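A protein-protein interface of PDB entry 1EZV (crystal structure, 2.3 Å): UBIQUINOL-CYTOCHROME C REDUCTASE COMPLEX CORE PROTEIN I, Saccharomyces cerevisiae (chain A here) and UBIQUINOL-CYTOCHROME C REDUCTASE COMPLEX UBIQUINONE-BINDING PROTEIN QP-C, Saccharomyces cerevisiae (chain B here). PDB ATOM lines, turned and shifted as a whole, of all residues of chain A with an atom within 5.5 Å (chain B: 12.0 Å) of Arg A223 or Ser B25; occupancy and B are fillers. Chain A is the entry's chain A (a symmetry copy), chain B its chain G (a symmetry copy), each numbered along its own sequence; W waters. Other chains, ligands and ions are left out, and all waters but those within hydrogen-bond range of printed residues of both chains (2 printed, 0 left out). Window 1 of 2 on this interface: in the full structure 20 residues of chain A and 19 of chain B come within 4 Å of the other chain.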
ATOM      1  N   GLU A 221     -19.703 -19.561  -6.547  1.00  0.00           N
ATOM      2  CA  GLU A 221     -21.027 -19.897  -7.059  1.00  0.00           C
ATOM      3  C   GLU A 221     -22.017 -18.774  -6.790  1.00  0.00           C
ATOM      4  O   GLU A 221     -21.828 -17.989  -5.865  1.00  0.00           O
ATOM      5  CB  GLU A 221     -21.536 -21.184  -6.407  1.00  0.00           C
ATOM      6  CG  GLU A 221     -21.594 -21.129  -4.874  1.00  0.00           C
ATOM      7  CD  GLU A 221     -22.127 -22.407  -4.249  1.00  0.00           C
ATOM      8  OE1 GLU A 221     -22.753 -22.328  -3.174  1.00  0.00           O
ATOM      9  OE2 GLU A 221     -21.912 -23.492  -4.823  1.00  0.00           O
ATOM     10  N   VAL A 222     -23.029 -18.665  -7.644  1.00  0.00           N
ATOM     11  CA  VAL A 222     -24.192 -17.829  -7.370  1.00  0.00           C
ATOM     12  C   VAL A 222     -25.440 -18.672  -7.624  1.00  0.00           C
ATOM     13  O   VAL A 222     -25.541 -19.351  -8.637  1.00  0.00           O
ATOM     14  CB  VAL A 222     -24.210 -16.538  -8.263  1.00  0.00           C
ATOM     15  CG1 VAL A 222     -24.017 -16.885  -9.741  1.00  0.00           C
ATOM     16  CG2 VAL A 222     -25.520 -15.781  -8.070  1.00  0.00           C
ATOM     17  N   ARG A 223     -26.322 -18.744  -6.636  1.00  0.00           N
ATOM     18  CA  ARG A 223     -27.468 -19.635  -6.732  1.00  0.00           C
ATOM     19  C   ARG A 223     -28.752 -18.816  -6.735  1.00  0.00           C
ATOM     20  O   ARG A 223     -29.017 -18.069  -5.802  1.00  0.00           O
ATOM     21  CB  ARG A 223     -27.436 -20.664  -5.582  1.00  0.00           C
ATOM     22  CG  ARG A 223     -26.349 -21.730  -5.780  1.00  0.00           C
ATOM     23  CD  ARG A 223     -25.815 -22.343  -4.479  1.00  0.00           C
ATOM     24  NE  ARG A 223     -26.306 -23.707  -4.312  1.00  0.00           N
ATOM     25  CZ  ARG A 223     -25.626 -24.815  -4.605  1.00  0.00           C
ATOM     26  NH1 ARG A 223     -26.291 -25.941  -4.756  1.00  0.00           N
ATOM     27  NH2 ARG A 223     -24.303 -24.857  -4.529  1.00  0.00           N
ATOM     28  N   LEU A 224     -29.426 -18.805  -7.881  1.00  0.00           N
ATOM     29  CA  LEU A 224     -30.609 -17.970  -8.080  1.00  0.00           C
ATOM     30  C   LEU A 224     -31.886 -18.802  -7.955  1.00  0.00           C
ATOM     31  O   LEU A 224     -32.700 -18.849  -8.871  1.00  0.00           O
ATOM     32  CB  LEU A 224     -30.541 -17.284  -9.459  1.00  0.00           C
ATOM     33  CG  LEU A 224     -29.277 -16.443  -9.714  1.00  0.00           C
ATOM     34  CD1 LEU A 224     -28.696 -16.753 -11.078  1.00  0.00           C
ATOM     35  CD2 LEU A 224     -29.601 -14.951  -9.602  1.00  0.00           C
ATOM     36  N   ARG A 225     -32.064 -19.434  -6.798  1.00  0.00           N
ATOM     37  CA  ARG A 225     -33.183 -20.349  -6.587  1.00  0.00           C
ATOM     38  C   ARG A 225     -34.502 -19.684  -6.906  1.00  0.00           C
ATOM     39  O   ARG A 225     -34.739 -18.554  -6.502  1.00  0.00           O
ATOM     40  CB  ARG A 225     -33.216 -20.855  -5.142  1.00  0.00           C
ATOM     41  CG  ARG A 225     -33.492 -22.345  -5.044  1.00  0.00           C
ATOM     42  CD  ARG A 225     -34.653 -22.690  -4.126  1.00  0.00           C
ATOM     43  NE  ARG A 225     -34.186 -23.446  -2.970  1.00  0.00           N
ATOM     44  CZ  ARG A 225     -34.915 -24.304  -2.266  1.00  0.00           C
ATOM     45  NH1 ARG A 225     -34.355 -24.944  -1.256  1.00  0.00           N
ATOM     46  NH2 ARG A 225     -36.192 -24.519  -2.545  1.00  0.00           N
ATOM     47  N   ILE A 406     -19.974 -22.054 -10.383  1.00  0.00           N
ATOM     48  CA  ILE A 406     -21.317 -22.603 -10.570  1.00  0.00           C
ATOM     49  C   ILE A 406     -22.336 -21.469 -10.601  1.00  0.00           C
ATOM     50  O   ILE A 406     -22.229 -20.524  -9.835  1.00  0.00           O
ATOM     51  CB  ILE A 406     -21.698 -23.585  -9.406  1.00  0.00           C
ATOM     52  CG1 ILE A 406     -20.621 -24.656  -9.239  1.00  0.00           C
ATOM     53  CG2 ILE A 406     -23.043 -24.252  -9.677  1.00  0.00           C
ATOM     54  CD1 ILE A 406     -20.855 -25.565  -8.066  1.00  0.00           C
ATOM     55  N   ALA A 407     -23.360 -21.609 -11.437  1.00  0.00           N
ATOM     56  CA  ALA A 407     -24.509 -20.713 -11.402  1.00  0.00           C
ATOM     57  C   ALA A 407     -25.754 -21.515 -11.724  1.00  0.00           C
ATOM     58  O   ALA A 407     -25.695 -22.435 -12.537  1.00  0.00           O
ATOM     59  CB  ALA A 407     -24.335 -19.594 -12.424  1.00  0.00           C
ATOM     60  N   GLY A 408     -26.886 -21.146 -11.128  1.00  0.00           N
ATOM     61  CA  GLY A 408     -28.121 -21.837 -11.450  1.00  0.00           C
ATOM     62  C   GLY A 408     -29.367 -21.054 -11.100  1.00  0.00           C
ATOM     63  O   GLY A 408     -29.317 -20.146 -10.283  1.00  0.00           O
ATOM     64  N   ILE A 412     -33.420 -25.556  -7.990  1.00  0.00           N
ATOM     65  CA  ILE A 412     -32.084 -26.084  -7.716  1.00  0.00           C
ATOM     66  C   ILE A 412     -31.835 -26.459  -6.238  1.00  0.00           C
ATOM     67  O   ILE A 412     -30.690 -26.445  -5.765  1.00  0.00           O
ATOM     68  CB  ILE A 412     -30.982 -25.093  -8.176  1.00  0.00           C
ATOM     69  CG1 ILE A 412     -31.207 -23.715  -7.556  1.00  0.00           C
ATOM     70  CG2 ILE A 412     -30.991 -24.967  -9.690  1.00  0.00           C
ATOM     71  CD1 ILE A 412     -30.071 -22.736  -7.819  1.00  0.00           C
ATOM     72  N   LEU A 415     -29.409 -29.326  -6.139  1.00  0.00           N
ATOM     73  CA  LEU A 415     -28.024 -29.104  -6.535  1.00  0.00           C
ATOM     74  C   LEU A 415     -27.245 -28.981  -5.244  1.00  0.00           C
ATOM     75  O   LEU A 415     -27.548 -28.128  -4.419  1.00  0.00           O
ATOM     76  CB  LEU A 415     -27.887 -27.820  -7.374  1.00  0.00           C
ATOM     77  CG  LEU A 415     -26.464 -27.401  -7.788  1.00  0.00           C
ATOM     78  CD1 LEU A 415     -25.952 -28.308  -8.894  1.00  0.00           C
ATOM     79  CD2 LEU A 415     -26.444 -25.954  -8.249  1.00  0.00           C
ATOM     80  N   LEU A 416     -26.404 -29.964  -4.973  1.00  0.00           N
ATOM     81  CA  LEU A 416     -25.740 -30.049  -3.679  1.00  0.00           C
ATOM     82  C   LEU A 416     -24.750 -28.904  -3.460  1.00  0.00           C
ATOM     83  O   LEU A 416     -24.496 -28.105  -4.362  1.00  0.00           O
ATOM     84  CB  LEU A 416     -25.037 -31.401  -3.556  1.00  0.00           C
ATOM     85  CG  LEU A 416     -25.768 -32.501  -2.770  1.00  0.00           C
ATOM     86  CD1 LEU A 416     -27.278 -32.344  -2.890  1.00  0.00           C
ATOM     87  CD2 LEU A 416     -25.315 -33.869  -3.251  1.00  0.00           C
ATOM     88  N   ASP A 417     -24.225 -28.808  -2.246  1.00  0.00           N
ATOM     89  CA  ASP A 417     -23.260 -27.774  -1.881  1.00  0.00           C
ATOM     90  C   ASP A 417     -22.015 -27.755  -2.764  1.00  0.00           C
ATOM     91  O   ASP A 417     -21.639 -28.761  -3.359  1.00  0.00           O
ATOM     92  CB  ASP A 417     -22.818 -27.972  -0.437  1.00  0.00           C
ATOM     93  CG  ASP A 417     -22.223 -29.333  -0.217  1.00  0.00           C
ATOM     94  OD1 ASP A 417     -22.999 -30.304  -0.283  1.00  0.00           O
ATOM     95  OD2 ASP A 417     -20.980 -29.447  -0.136  1.00  0.00           O
ATOM     96  N   TYR A 418     -21.278 -26.658  -2.658  1.00  0.00           N
ATOM     97  CA  TYR A 418     -20.089 -26.442  -3.456  1.00  0.00           C
ATOM     98  C   TYR A 418     -19.082 -27.568  -3.290  1.00  0.00           C
ATOM     99  O   TYR A 418     -18.661 -28.163  -4.278  1.00  0.00           O
ATOM    100  CB  TYR A 418     -19.444 -25.103  -3.086  1.00  0.00           C
ATOM    101  CG  TYR A 418     -18.289 -24.730  -3.988  1.00  0.00           C
ATOM    102  CD1 TYR A 418     -18.514 -24.090  -5.210  1.00  0.00           C
ATOM    103  CD2 TYR A 418     -16.973 -25.044  -3.635  1.00  0.00           C
ATOM    104  CE1 TYR A 418     -17.455 -23.763  -6.054  1.00  0.00           C
ATOM    105  CE2 TYR A 418     -15.911 -24.738  -4.476  1.00  0.00           C
ATOM    106  CZ  TYR A 418     -16.161 -24.091  -5.686  1.00  0.00           C
ATOM    107  OH  TYR A 418     -15.117 -23.794  -6.530  1.00  0.00           O
ATOM    108  N   TRP B  12     -33.884 -34.125  -0.992  1.00  0.00           N
ATOM    109  CA  TRP B  12     -33.375 -33.191  -1.995  1.00  0.00           C
ATOM    110  C   TRP B  12     -34.285 -33.059  -3.216  1.00  0.00           C
ATOM    111  O   TRP B  12     -34.610 -34.056  -3.877  1.00  0.00           O
ATOM    112  CB  TRP B  12     -31.981 -33.626  -2.440  1.00  0.00           C
ATOM    113  CG  TRP B  12     -31.020 -33.725  -1.308  1.00  0.00           C
ATOM    114  CD1 TRP B  12     -30.496 -34.862  -0.781  1.00  0.00           C
ATOM    115  CD2 TRP B  12     -30.459 -32.637  -0.564  1.00  0.00           C
ATOM    116  NE1 TRP B  12     -29.634 -34.554   0.244  1.00  0.00           N
ATOM    117  CE2 TRP B  12     -29.587 -33.197   0.394  1.00  0.00           C
ATOM    118  CE3 TRP B  12     -30.598 -31.243  -0.623  1.00  0.00           C
ATOM    119  CZ2 TRP B  12     -28.842 -32.404   1.289  1.00  0.00           C
ATOM    120  CZ3 TRP B  12     -29.854 -30.453   0.264  1.00  0.00           C
ATOM    121  CH2 TRP B  12     -28.985 -31.040   1.202  1.00  0.00           C
ATOM    122  N   GLY B  13     -34.767 -31.838  -3.449  1.00  0.00           N
ATOM    123  CA  GLY B  13     -35.693 -31.605  -4.542  1.00  0.00           C
ATOM    124  C   GLY B  13     -37.144 -31.530  -4.092  1.00  0.00           C
ATOM    125  O   GLY B  13     -37.989 -30.997  -4.819  1.00  0.00           O
ATOM    126  N   MET B  15     -38.001 -31.029  -0.244  1.00  0.00           N
ATOM    127  CA  MET B  15     -37.716 -31.025   1.186  1.00  0.00           C
ATOM    128  C   MET B  15     -38.958 -30.764   2.019  1.00  0.00           C
ATOM    129  O   MET B  15     -39.020 -31.162   3.186  1.00  0.00           O
ATOM    130  CB  MET B  15     -36.652 -29.982   1.519  1.00  0.00           C
ATOM    131  CG  MET B  15     -35.841 -30.329   2.760  1.00  0.00           C
ATOM    132  SD  MET B  15     -34.853 -31.823   2.527  1.00  0.00           S
ATOM    133  CE  MET B  15     -33.505 -31.171   1.542  1.00  0.00           C
ATOM    134  N   GLN B  20     -39.451 -21.044  -2.701  1.00  0.00           N
ATOM    135  CA  GLN B  20     -38.494 -19.961  -2.502  1.00  0.00           C
ATOM    136  C   GLN B  20     -38.315 -19.185  -3.794  1.00  0.00           C
ATOM    137  O   GLN B  20     -38.134 -19.774  -4.856  1.00  0.00           O
ATOM    138  CB  GLN B  20     -37.134 -20.511  -2.042  1.00  0.00           C
ATOM    139  CG  GLN B  20     -37.119 -21.082  -0.627  1.00  0.00           C
ATOM    140  CD  GLN B  20     -35.741 -21.567  -0.208  1.00  0.00           C
ATOM    141  OE1 GLN B  20     -34.725 -21.025  -0.641  1.00  0.00           O
ATOM    142  NE2 GLN B  20     -35.698 -22.597   0.631  1.00  0.00           N
ATOM    143  N   LYS B  21     -38.386 -17.862  -3.697  1.00  0.00           N
ATOM    144  CA  LYS B  21     -38.211 -16.978  -4.844  1.00  0.00           C
ATOM    145  C   LYS B  21     -37.629 -15.664  -4.338  1.00  0.00           C
ATOM    146  O   LYS B  21     -37.985 -15.206  -3.253  1.00  0.00           O
ATOM    147  CB  LYS B  21     -39.561 -16.723  -5.514  1.00  0.00           C
ATOM    148  CG  LYS B  21     -39.490 -15.975  -6.844  1.00  0.00           C
ATOM    149  CD  LYS B  21     -40.901 -15.723  -7.391  1.00  0.00           C
ATOM    150  CE  LYS B  21     -40.922 -15.605  -8.908  1.00  0.00           C
ATOM    151  NZ  LYS B  21     -39.990 -14.560  -9.391  1.00  0.00           N
ATOM    152  N   GLY B  22     -36.670 -15.112  -5.075  1.00  0.00           N
ATOM    153  CA  GLY B  22     -36.123 -13.816  -4.728  1.00  0.00           C
ATOM    154  C   GLY B  22     -34.840 -13.851  -3.921  1.00  0.00           C
ATOM    155  O   GLY B  22     -34.148 -12.833  -3.810  1.00  0.00           O
ATOM    156  N   ILE B  23     -34.557 -14.987  -3.288  1.00  0.00           N
ATOM    157  CA  ILE B  23     -33.329 -15.143  -2.506  1.00  0.00           C
ATOM    158  C   ILE B  23     -32.201 -15.639  -3.411  1.00  0.00           C
ATOM    159  O   ILE B  23     -32.362 -16.623  -4.131  1.00  0.00           O
ATOM    160  CB  ILE B  23     -33.529 -16.150  -1.349  1.00  0.00           C
ATOM    161  CG1 ILE B  23     -34.707 -15.711  -0.475  1.00  0.00           C
ATOM    162  CG2 ILE B  23     -32.249 -16.270  -0.522  1.00  0.00           C
ATOM    163  CD1 ILE B  23     -35.375 -16.840   0.288  1.00  0.00           C
ATOM    164  N   THR B  24     -31.072 -14.944  -3.375  1.00  0.00           N
ATOM    165  CA  THR B  24     -29.904 -15.303  -4.168  1.00  0.00           C
ATOM    166  C   THR B  24     -28.722 -15.482  -3.221  1.00  0.00           C
ATOM    167  O   THR B  24     -28.447 -14.603  -2.403  1.00  0.00           O
ATOM    168  CB  THR B  24     -29.576 -14.178  -5.190  1.00  0.00           C
ATOM    169  OG1 THR B  24     -30.665 -14.050  -6.110  1.00  0.00           O
ATOM    170  CG2 THR B  24     -28.300 -14.477  -5.963  1.00  0.00           C
ATOM    171  N   SER B  25     -28.025 -16.613  -3.319  1.00  0.00           N
ATOM    172  CA  SER B  25     -26.897 -16.856  -2.426  1.00  0.00           C
ATOM    173  C   SER B  25     -25.578 -16.873  -3.167  1.00  0.00           C
ATOM    174  O   SER B  25     -25.529 -17.155  -4.360  1.00  0.00           O
ATOM    175  CB  SER B  25     -27.085 -18.169  -1.659  1.00  0.00           C
ATOM    176  OG  SER B  25     -26.985 -19.286  -2.521  1.00  0.00           O
ATOM    177  N   TYR B  26     -24.509 -16.548  -2.454  1.00  0.00           N
ATOM    178  CA  TYR B  26     -23.178 -16.496  -3.044  1.00  0.00           C
ATOM    179  C   TYR B  26     -22.213 -17.200  -2.108  1.00  0.00           C
ATOM    180  O   TYR B  26     -22.344 -17.085  -0.888  1.00  0.00           O
ATOM    181  CB  TYR B  26     -22.719 -15.042  -3.225  1.00  0.00           C
ATOM    182  CG  TYR B  26     -23.629 -14.188  -4.083  1.00  0.00           C
ATOM    183  CD1 TYR B  26     -24.750 -13.564  -3.536  1.00  0.00           C
ATOM    184  CD2 TYR B  26     -23.319 -13.929  -5.420  1.00  0.00           C
ATOM    185  CE1 TYR B  26     -25.535 -12.707  -4.293  1.00  0.00           C
ATOM    186  CE2 TYR B  26     -24.092 -13.057  -6.184  1.00  0.00           C
ATOM    187  CZ  TYR B  26     -25.197 -12.452  -5.615  1.00  0.00           C
ATOM    188  OH  TYR B  26     -25.965 -11.579  -6.357  1.00  0.00           O
ATOM    189  N   ALA B  27     -21.203 -17.855  -2.671  1.00  0.00           N
ATOM    190  CA  ALA B  27     -20.148 -18.443  -1.861  1.00  0.00           C
ATOM    191  C   ALA B  27     -18.846 -18.538  -2.649  1.00  0.00           C
ATOM    192  O   ALA B  27     -18.845 -18.443  -3.874  1.00  0.00           O
ATOM    193  CB  ALA B  27     -20.578 -19.837  -1.360  1.00  0.00           C
ATOM    194  N   VAL B  28     -17.761 -18.842  -1.944  1.00  0.00           N
ATOM    195  CA  VAL B  28     -16.435 -18.872  -2.537  1.00  0.00           C
ATOM    196  C   VAL B  28     -15.691 -20.110  -2.042  1.00  0.00           C
ATOM    197  O   VAL B  28     -15.712 -20.416  -0.847  1.00  0.00           O
ATOM    198  CB  VAL B  28     -15.630 -17.593  -2.155  1.00  0.00           C
ATOM    199  CG1 VAL B  28     -14.154 -17.773  -2.487  1.00  0.00           C
ATOM    200  CG2 VAL B  28     -16.183 -16.384  -2.905  1.00  0.00           C
ATOM    201  N   SER B  29     -15.000 -20.787  -2.955  1.00  0.00           N
ATOM    202  CA  SER B  29     -14.275 -22.008  -2.632  1.00  0.00           C
ATOM    203  C   SER B  29     -13.378 -21.823  -1.411  1.00  0.00           C
ATOM    204  O   SER B  29     -12.699 -20.799  -1.274  1.00  0.00           O
ATOM    205  CB  SER B  29     -13.429 -22.462  -3.822  1.00  0.00           C
ATOM    206  OG  SER B  29     -12.605 -23.567  -3.477  1.00  0.00           O
ATOM    207  N   PRO B  30     -13.422 -22.788  -0.474  1.00  0.00           N
ATOM    208  CA  PRO B  30     -12.452 -22.889   0.620  1.00  0.00           C
ATOM    209  C   PRO B  30     -11.020 -22.835   0.115  1.00  0.00           C
ATOM    210  O   PRO B  30     -10.137 -22.336   0.804  1.00  0.00           O
ATOM    211  CB  PRO B  30     -12.775 -24.240   1.253  1.00  0.00           C
ATOM    212  CG  PRO B  30     -14.243 -24.385   1.021  1.00  0.00           C
ATOM    213  CD  PRO B  30     -14.478 -23.812  -0.356  1.00  0.00           C
HETATM  214  O   HOH W   1     -35.090 -17.915  -3.868  1.00  0.00           O
HETATM  215  O   HOH W   2     -19.688 -15.651  -5.271  1.00  0.00           O
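OE2 of Glu A221 is in salt-bridge range of NH2 of Arg A223 (2.8 Å).
The backbone NH (N) of Val A222 sits at hydrogen-bond distance from the backbone carbonyl oxygen (O) of Ile A406 (3.0 Å).
The backbone NH (N) of Gly A408 sits at hydrogen-bond distance from the backbone carbonyl oxygen (O) of Val A222, at 3.4 Å.
The guanidinium group (NH1) of Arg A223 lies within hydrogen-bond range of the backbone carbonyl oxygen (O) of Leu A415 (2.5 Å).
NH1 of Arg A223 lies within hydrogen-bond range of O of Leu A416, at 2.8 Å.
N of Leu A224 lies within hydrogen-bond range of O of Gly A408 (2.8 Å).
Of the 13 printed residues of chain A, 7 touch a printed residue of chain B.
Printed residues of chain A that touch a printed residue of chain B: Glu A221, Val A222, Arg A223, Leu A224, Arg A225, Leu A416 and Tyr A418.
Hydrophobic or aromatic side chains of chain B that line the printed part of chain A: Trp B12, Tyr B26 and Ala B27.
Along chain B the printed residues that touch a printed residue of chain A span positions 12 to 29.
Among the printed residues, no Asp or Glu carboxylate lies within 4 Å of a Lys or Arg side-chain nitrogen of the other chain.
The backbone carbonyl oxygen (O) of Ala B27 is in hydrogen-bond range of the backbone NH (N) of Glu A221, at 3.0 Å.
The backbone NH of Arg A223 sits at hydrogen-bond distance from the backbone carbonyl oxygen of Ser B25.
NH1 of Arg A225 sits close to NE2 of Gln B20, 3.3 Å away.
CA of Tyr B26 touches O of Glu A221, at 3.5 Å.
Thr B24 touches Val A222.
CA of Val A222 touches O of Ser B25 (3.4 Å).
Val A222 touches Tyr B26.
Arg A223 touches Thr B24 (O to CA, 3.3 Å).
Leu A224 touches Thr B24.
O of Ile B23 touches O of Arg A225 (3.9 Å).
CD1 of Leu A416 touches CD2 of Trp B12, 3.95 Å away.
CE2 of Tyr A418 touches CB of Ser B29, 3.4 Å away.
Of chain B, only Tyr B26 and Ala B27 come within 4 Å of Glu A221.
Val A222 touches just these residues of chain B: Thr B24 (3.7 Å), Ser B25 (3.4 Å) and Tyr B26 (3.6 Å).
Printed residues of chain B within 4 Å of Arg A223: Thr B24 and Ser B25.
Leu A224 touches just one residue of chain B: Thr B24.
No residue of chain B comes within 4 Å of Ala A407.
No residue of chain B comes within 4 Å of Gly A408.
No residue of chain B comes within 4 Å of Ile A412.
Leu A415 touches none of the printed residues of chain B.
Printed residues of chain B within 4 Å of Leu A416: Trp B12 (3.95 Å).
Of the printed residues of chain B, Tyr A418 touches Ser B29.
Of the printed residues of chain A, Gln B20 touches Arg A225 (3.3 Å).
Lys B21 touches none of the printed residues of chain A.
Printed residues of chain A within 4 Å of Thr B24: Val A222 (3.7 Å), Arg A223 (3.3 Å) and Leu A224 (3.8 Å).
Of the printed residues of chain A, Ser B25 touches Val A222 (3.4 Å) and Arg A223 (2.9 Å).
Printed residues of chain A within 4 Å of Ala B27: Glu A221.
The nearest printed residue of chain B that does not touch Arg A225 is Lys B21 (4.2 Å).
Water W1 lies within hydrogen-bond range of the backbone carbonyl oxygen (O) of Arg A225, the backbone carbonyl oxygen (O) of Ile B23, the backbone NH (N) of Lys B21 and the backbone NH (N) of Gly B22.
Water W2 lies within hydrogen-bond range of the backbone carbonyl oxygen of Glu A221 (3.2 Å) and the backbone carbonyl oxygen of Ala B27 (3.2 Å).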
